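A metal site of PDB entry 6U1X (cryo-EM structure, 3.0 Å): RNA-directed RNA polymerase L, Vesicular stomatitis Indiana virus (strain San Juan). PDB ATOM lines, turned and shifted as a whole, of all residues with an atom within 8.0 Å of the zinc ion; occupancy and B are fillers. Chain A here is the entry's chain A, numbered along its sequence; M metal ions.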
ATOM      1  N   THR A 905     -11.193  13.595  -6.588  1.00  0.00           N
ATOM      2  CA  THR A 905     -10.614  13.783  -7.914  1.00  0.00           C
ATOM      3  C   THR A 905      -9.160  13.338  -7.965  1.00  0.00           C
ATOM      4  O   THR A 905      -8.713  12.864  -9.019  1.00  0.00           O
ATOM      5  CB  THR A 905     -10.736  15.243  -8.337  1.00  0.00           C
ATOM      6  OG1 THR A 905     -12.081  15.689  -8.146  1.00  0.00           O
ATOM      7  CG2 THR A 905     -10.361  15.402  -9.792  1.00  0.00           C
ATOM      8  N   SER A 909      -8.152  10.681 -10.817  1.00  0.00           N
ATOM      9  CA  SER A 909      -7.093  11.009 -11.759  1.00  0.00           C
ATOM     10  C   SER A 909      -5.965   9.992 -11.689  1.00  0.00           C
ATOM     11  O   SER A 909      -5.405   9.601 -12.715  1.00  0.00           O
ATOM     12  CB  SER A 909      -6.569  12.414 -11.484  1.00  0.00           C
ATOM     13  OG  SER A 909      -7.623  13.361 -11.443  1.00  0.00           O
ATOM     14  N   ARG A 912      -7.156   6.712 -13.363  1.00  0.00           N
ATOM     15  CA  ARG A 912      -7.210   6.880 -14.810  1.00  0.00           C
ATOM     16  C   ARG A 912      -5.811   6.925 -15.406  1.00  0.00           C
ATOM     17  O   ARG A 912      -5.574   6.352 -16.479  1.00  0.00           O
ATOM     18  CB  ARG A 912      -7.968   8.157 -15.181  1.00  0.00           C
ATOM     19  CG  ARG A 912      -7.889   8.474 -16.661  1.00  0.00           C
ATOM     20  CD  ARG A 912      -8.985   9.387 -17.126  1.00  0.00           C
ATOM     21  NE  ARG A 912      -8.879   9.619 -18.562  1.00  0.00           N
ATOM     22  CZ  ARG A 912      -9.261   8.745 -19.501  1.00  0.00           C
ATOM     23  NH1 ARG A 912      -9.796   7.581 -19.169  1.00  0.00           N
ATOM     24  NH2 ARG A 912      -9.108   9.056 -20.781  1.00  0.00           N
ATOM     25  N   TRP A1079     -14.113   5.809 -17.198  1.00  0.00           N
ATOM     26  CA  TRP A1079     -14.576   7.170 -17.408  1.00  0.00           C
ATOM     27  C   TRP A1079     -13.539   7.974 -18.172  1.00  0.00           C
ATOM     28  O   TRP A1079     -12.339   7.702 -18.096  1.00  0.00           O
ATOM     29  CB  TRP A1079     -14.882   7.856 -16.071  1.00  0.00           C
ATOM     30  CG  TRP A1079     -13.677   8.050 -15.214  1.00  0.00           C
ATOM     31  CD1 TRP A1079     -12.911   9.174 -15.124  1.00  0.00           C
ATOM     32  CD2 TRP A1079     -13.092   7.102 -14.310  1.00  0.00           C
ATOM     33  NE1 TRP A1079     -11.891   8.976 -14.232  1.00  0.00           N
ATOM     34  CE2 TRP A1079     -11.982   7.710 -13.721  1.00  0.00           C
ATOM     35  CE3 TRP A1079     -13.415   5.789 -13.954  1.00  0.00           C
ATOM     36  CZ2 TRP A1079     -11.187   7.058 -12.786  1.00  0.00           C
ATOM     37  CZ3 TRP A1079     -12.617   5.148 -13.027  1.00  0.00           C
ATOM     38  CH2 TRP A1079     -11.515   5.784 -12.453  1.00  0.00           C
ATOM     39  N   THR A1080     -14.006   8.989 -18.905  1.00  0.00           N
ATOM     40  CA  THR A1080     -13.111   9.815 -19.701  1.00  0.00           C
ATOM     41  C   THR A1080     -12.439  10.890 -18.854  1.00  0.00           C
ATOM     42  O   THR A1080     -11.216  10.947 -18.759  1.00  0.00           O
ATOM     43  CB  THR A1080     -13.886  10.447 -20.857  1.00  0.00           C
ATOM     44  OG1 THR A1080     -14.546   9.419 -21.608  1.00  0.00           O
ATOM     45  CG2 THR A1080     -12.958  11.217 -21.766  1.00  0.00           C
ATOM     46  N   CYS A1081     -13.246  11.764 -18.242  1.00  0.00           N
ATOM     47  CA  CYS A1081     -12.755  12.851 -17.408  1.00  0.00           C
ATOM     48  C   CYS A1081     -13.037  12.541 -15.946  1.00  0.00           C
ATOM     49  O   CYS A1081     -14.124  12.066 -15.598  1.00  0.00           O
ATOM     50  CB  CYS A1081     -13.403  14.179 -17.784  1.00  0.00           C
ATOM     51  SG  CYS A1081     -12.541  15.643 -17.151  1.00  0.00           S
ATOM     52  N   SER A1082     -12.043  12.812 -15.088  1.00  0.00           N
ATOM     53  CA  SER A1082     -12.219  12.530 -13.666  1.00  0.00           C
ATOM     54  C   SER A1082     -13.119  13.555 -12.996  1.00  0.00           C
ATOM     55  O   SER A1082     -13.854  13.222 -12.068  1.00  0.00           O
ATOM     56  CB  SER A1082     -10.856  12.514 -12.983  1.00  0.00           C
ATOM     57  OG  SER A1082      -9.975  11.598 -13.621  1.00  0.00           O
ATOM     58  N   ALA A1083     -13.086  14.807 -13.465  1.00  0.00           N
ATOM     59  CA  ALA A1083     -13.928  15.836 -12.865  1.00  0.00           C
ATOM     60  C   ALA A1083     -15.400  15.583 -13.169  1.00  0.00           C
ATOM     61  O   ALA A1083     -16.251  15.663 -12.279  1.00  0.00           O
ATOM     62  CB  ALA A1083     -13.498  17.206 -13.382  1.00  0.00           C
ATOM     63  N   THR A1084     -15.715  15.290 -14.434  1.00  0.00           N
ATOM     64  CA  THR A1084     -17.095  14.977 -14.793  1.00  0.00           C
ATOM     65  C   THR A1084     -17.573  13.724 -14.071  1.00  0.00           C
ATOM     66  O   THR A1084     -18.731  13.646 -13.651  1.00  0.00           O
ATOM     67  CB  THR A1084     -17.211  14.805 -16.303  1.00  0.00           C
ATOM     68  OG1 THR A1084     -16.676  15.950 -16.975  1.00  0.00           O
ATOM     69  CG2 THR A1084     -18.659  14.618 -16.705  1.00  0.00           C
ATOM     70  N   HIS A1085     -16.703  12.731 -13.944  1.00  0.00           N
ATOM     71  CA  HIS A1085     -17.090  11.512 -13.246  1.00  0.00           C
ATOM     72  C   HIS A1085     -17.362  11.795 -11.778  1.00  0.00           C
ATOM     73  O   HIS A1085     -18.327  11.276 -11.212  1.00  0.00           O
ATOM     74  CB  HIS A1085     -15.999  10.448 -13.383  1.00  0.00           C
ATOM     75  CG  HIS A1085     -16.451   9.079 -12.999  1.00  0.00           C
ATOM     76  ND1 HIS A1085     -17.568   8.481 -13.552  1.00  0.00           N
ATOM     77  CD2 HIS A1085     -15.951   8.191 -12.111  1.00  0.00           C
ATOM     78  CE1 HIS A1085     -17.726   7.280 -13.017  1.00  0.00           C
ATOM     79  NE2 HIS A1085     -16.759   7.077 -12.156  1.00  0.00           N
ATOM     80  N   PRO A1104     -10.610  20.048 -10.388  1.00  0.00           N
ATOM     81  CA  PRO A1104      -9.815  19.155 -11.233  1.00  0.00           C
ATOM     82  C   PRO A1104      -8.360  19.106 -10.806  1.00  0.00           C
ATOM     83  O   PRO A1104      -7.750  20.131 -10.484  1.00  0.00           O
ATOM     84  CB  PRO A1104      -9.977  19.771 -12.627  1.00  0.00           C
ATOM     85  CG  PRO A1104     -10.150  21.193 -12.361  1.00  0.00           C
ATOM     86  CD  PRO A1104     -10.952  21.285 -11.108  1.00  0.00           C
ATOM     87  N   HIS A1105      -7.801  17.900 -10.839  1.00  0.00           N
ATOM     88  CA  HIS A1105      -6.419  17.686 -10.412  1.00  0.00           C
ATOM     89  C   HIS A1105      -5.471  17.874 -11.586  1.00  0.00           C
ATOM     90  O   HIS A1105      -5.836  17.591 -12.733  1.00  0.00           O
ATOM     91  CB  HIS A1105      -6.263  16.291  -9.831  1.00  0.00           C
ATOM     92  CG  HIS A1105      -4.989  16.087  -9.075  1.00  0.00           C
ATOM     93  ND1 HIS A1105      -3.904  15.436  -9.616  1.00  0.00           N
ATOM     94  CD2 HIS A1105      -4.626  16.465  -7.832  1.00  0.00           C
ATOM     95  CE1 HIS A1105      -2.924  15.415  -8.722  1.00  0.00           C
ATOM     96  NE2 HIS A1105      -3.334  16.035  -7.635  1.00  0.00           N
ATOM     97  N   LEU A1107      -3.141  16.088 -12.659  1.00  0.00           N
ATOM     98  CA  LEU A1107      -2.515  14.868 -13.145  1.00  0.00           C
ATOM     99  C   LEU A1107      -3.005  14.493 -14.540  1.00  0.00           C
ATOM    100  O   LEU A1107      -2.247  13.923 -15.326  1.00  0.00           O
ATOM    101  CB  LEU A1107      -2.760  13.716 -12.179  1.00  0.00           C
ATOM    102  CG  LEU A1107      -2.011  12.420 -12.452  1.00  0.00           C
ATOM    103  CD1 LEU A1107      -0.515  12.622 -12.410  1.00  0.00           C
ATOM    104  CD2 LEU A1107      -2.433  11.365 -11.453  1.00  0.00           C
ATOM    105  N   GLU A1108      -4.267  14.794 -14.855  1.00  0.00           N
ATOM    106  CA  GLU A1108      -4.808  14.624 -16.198  1.00  0.00           C
ATOM    107  C   GLU A1108      -5.054  15.949 -16.902  1.00  0.00           C
ATOM    108  O   GLU A1108      -4.987  16.000 -18.133  1.00  0.00           O
ATOM    109  CB  GLU A1108      -6.108  13.834 -16.172  1.00  0.00           C
ATOM    110  CG  GLU A1108      -7.222  14.432 -15.341  1.00  0.00           C
ATOM    111  CD  GLU A1108      -8.574  13.837 -15.668  1.00  0.00           C
ATOM    112  OE1 GLU A1108      -8.747  12.624 -15.458  1.00  0.00           O
ATOM    113  OE2 GLU A1108      -9.444  14.584 -16.153  1.00  0.00           O
ATOM    114  N   MET A1109      -5.344  17.008 -16.153  1.00  0.00           N
ATOM    115  CA  MET A1109      -5.532  18.322 -16.748  1.00  0.00           C
ATOM    116  C   MET A1109      -4.265  18.784 -17.459  1.00  0.00           C
ATOM    117  O   MET A1109      -4.342  19.401 -18.527  1.00  0.00           O
ATOM    118  CB  MET A1109      -5.946  19.314 -15.658  1.00  0.00           C
ATOM    119  CG  MET A1109      -5.688  20.765 -15.987  1.00  0.00           C
ATOM    120  SD  MET A1109      -6.501  21.888 -14.853  1.00  0.00           S
ATOM    121  CE  MET A1109      -5.700  23.401 -15.332  1.00  0.00           C
ATOM    122  N   LEU A1110      -3.100  18.505 -16.881  1.00  0.00           N
ATOM    123  CA  LEU A1110      -1.821  18.828 -17.480  1.00  0.00           C
ATOM    124  C   LEU A1110      -1.116  17.607 -18.059  1.00  0.00           C
ATOM    125  O   LEU A1110      -0.591  17.671 -19.168  1.00  0.00           O
ATOM    126  CB  LEU A1110      -0.900  19.489 -16.450  1.00  0.00           C
ATOM    127  CG  LEU A1110      -1.356  20.840 -15.893  1.00  0.00           C
ATOM    128  CD1 LEU A1110      -0.472  21.244 -14.748  1.00  0.00           C
ATOM    129  CD2 LEU A1110      -1.345  21.895 -16.962  1.00  0.00           C
ATOM    130  N   ALA A1298      -3.902  19.036 -21.378  1.00  0.00           N
ATOM    131  CA  ALA A1298      -4.180  17.802 -22.096  1.00  0.00           C
ATOM    132  C   ALA A1298      -5.670  17.498 -22.140  1.00  0.00           C
ATOM    133  O   ALA A1298      -6.256  17.353 -23.218  1.00  0.00           O
ATOM    134  CB  ALA A1298      -3.416  16.637 -21.453  1.00  0.00           C
ATOM    135  N   CYS A1299      -6.289  17.399 -20.971  1.00  0.00           N
ATOM    136  CA  CYS A1299      -7.725  17.114 -20.865  1.00  0.00           C
ATOM    137  C   CYS A1299      -8.451  18.442 -20.787  1.00  0.00           C
ATOM    138  O   CYS A1299      -8.637  19.019 -19.711  1.00  0.00           O
ATOM    139  CB  CYS A1299      -8.012  16.236 -19.659  1.00  0.00           C
ATOM    140  SG  CYS A1299      -9.682  15.554 -19.583  1.00  0.00           S
ATOM    141  N   LYS A1300      -8.890  18.947 -21.945  1.00  0.00           N
ATOM    142  CA  LYS A1300      -9.579  20.220 -22.003  1.00  0.00           C
ATOM    143  C   LYS A1300     -10.962  20.159 -21.372  1.00  0.00           C
ATOM    144  O   LYS A1300     -11.545  21.219 -21.102  1.00  0.00           O
ATOM    145  CB  LYS A1300      -9.703  20.679 -23.450  1.00  0.00           C
ATOM    146  CG  LYS A1300      -8.369  20.807 -24.172  1.00  0.00           C
ATOM    147  CD  LYS A1300      -8.498  21.506 -25.524  1.00  0.00           C
ATOM    148  CE  LYS A1300      -9.390  20.731 -26.501  1.00  0.00           C
ATOM    149  NZ  LYS A1300      -8.938  19.335 -26.708  1.00  0.00           N
ATOM    150  N   SER A1301     -11.496  18.961 -21.123  1.00  0.00           N
ATOM    151  CA  SER A1301     -12.830  18.861 -20.538  1.00  0.00           C
ATOM    152  C   SER A1301     -12.855  19.387 -19.111  1.00  0.00           C
ATOM    153  O   SER A1301     -13.873  19.939 -18.678  1.00  0.00           O
ATOM    154  CB  SER A1301     -13.310  17.413 -20.566  1.00  0.00           C
ATOM    155  OG  SER A1301     -14.630  17.303 -20.088  1.00  0.00           O
ATOM    156  N   CYS A1302     -11.766  19.236 -18.362  1.00  0.00           N
ATOM    157  CA  CYS A1302     -11.697  19.693 -16.976  1.00  0.00           C
ATOM    158  C   CYS A1302     -11.124  21.116 -16.905  1.00  0.00           C
ATOM    159  O   CYS A1302     -10.101  21.379 -16.284  1.00  0.00           O
ATOM    160  CB  CYS A1302     -10.897  18.719 -16.126  1.00  0.00           C
ATOM    161  SG  CYS A1302      -9.427  18.054 -16.892  1.00  0.00           S
ATOM    162  N   LEU A1303     -11.814  22.020 -17.591  1.00  0.00           N
ATOM    163  CA  LEU A1303     -11.622  23.455 -17.458  1.00  0.00           C
ATOM    164  C   LEU A1303     -12.735  24.114 -16.666  1.00  0.00           C
ATOM    165  O   LEU A1303     -12.453  24.989 -15.846  1.00  0.00           O
ATOM    166  CB  LEU A1303     -11.500  24.118 -18.838  1.00  0.00           C
ATOM    167  CG  LEU A1303     -10.234  23.791 -19.624  1.00  0.00           C
ATOM    168  CD1 LEU A1303     -10.311  24.357 -21.038  1.00  0.00           C
ATOM    169  CD2 LEU A1303      -9.002  24.320 -18.914  1.00  0.00           C
ATOM    170  N   ARG A1304     -13.980  23.707 -16.898  1.00  0.00           N
ATOM    171  CA  ARG A1304     -15.124  24.038 -16.052  1.00  0.00           C
ATOM    172  C   ARG A1304     -15.241  25.526 -15.780  1.00  0.00           C
ATOM    173  O   ARG A1304     -14.969  25.980 -14.661  1.00  0.00           O
ATOM    174  CB  ARG A1304     -15.012  23.282 -14.724  1.00  0.00           C
ATOM    175  CG  ARG A1304     -15.131  21.763 -14.867  1.00  0.00           C
ATOM    176  CD  ARG A1304     -14.860  21.071 -13.542  1.00  0.00           C
ATOM    177  NE  ARG A1304     -15.733  21.543 -12.478  1.00  0.00           N
ATOM    178  CZ  ARG A1304     -16.969  21.108 -12.254  1.00  0.00           C
ATOM    179  NH1 ARG A1304     -17.515  20.173 -13.013  1.00  0.00           N
ATOM    180  NH2 ARG A1304     -17.669  21.626 -11.251  1.00  0.00           N
HETATM  181 ZN    ZN M   1     -10.254  15.919 -17.382  1.00  0.00          ZN
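The side-chain carboxylate (OE1) of Glu 1108 sits at hydrogen-bond distance from the side-chain hydroxyl (OG) of Ser 1082 (2.4 Å).
The nearest printed residue that does not touch the zinc ion is Ser 1082 (4.3 Å).
The zinc ion is bound by the side-chain carboxylate (OE2) of Glu 1108 (2.0 Å), the side-chain sulfur (SG) of Cys 1299 (2.3 Å), the side-chain sulfur (SG) of Cys 1081 (2.3 Å) and the side-chain sulfur (SG) of Cys 1302 (2.3 Å).
The zinc ion has four donor atoms within binding distance.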
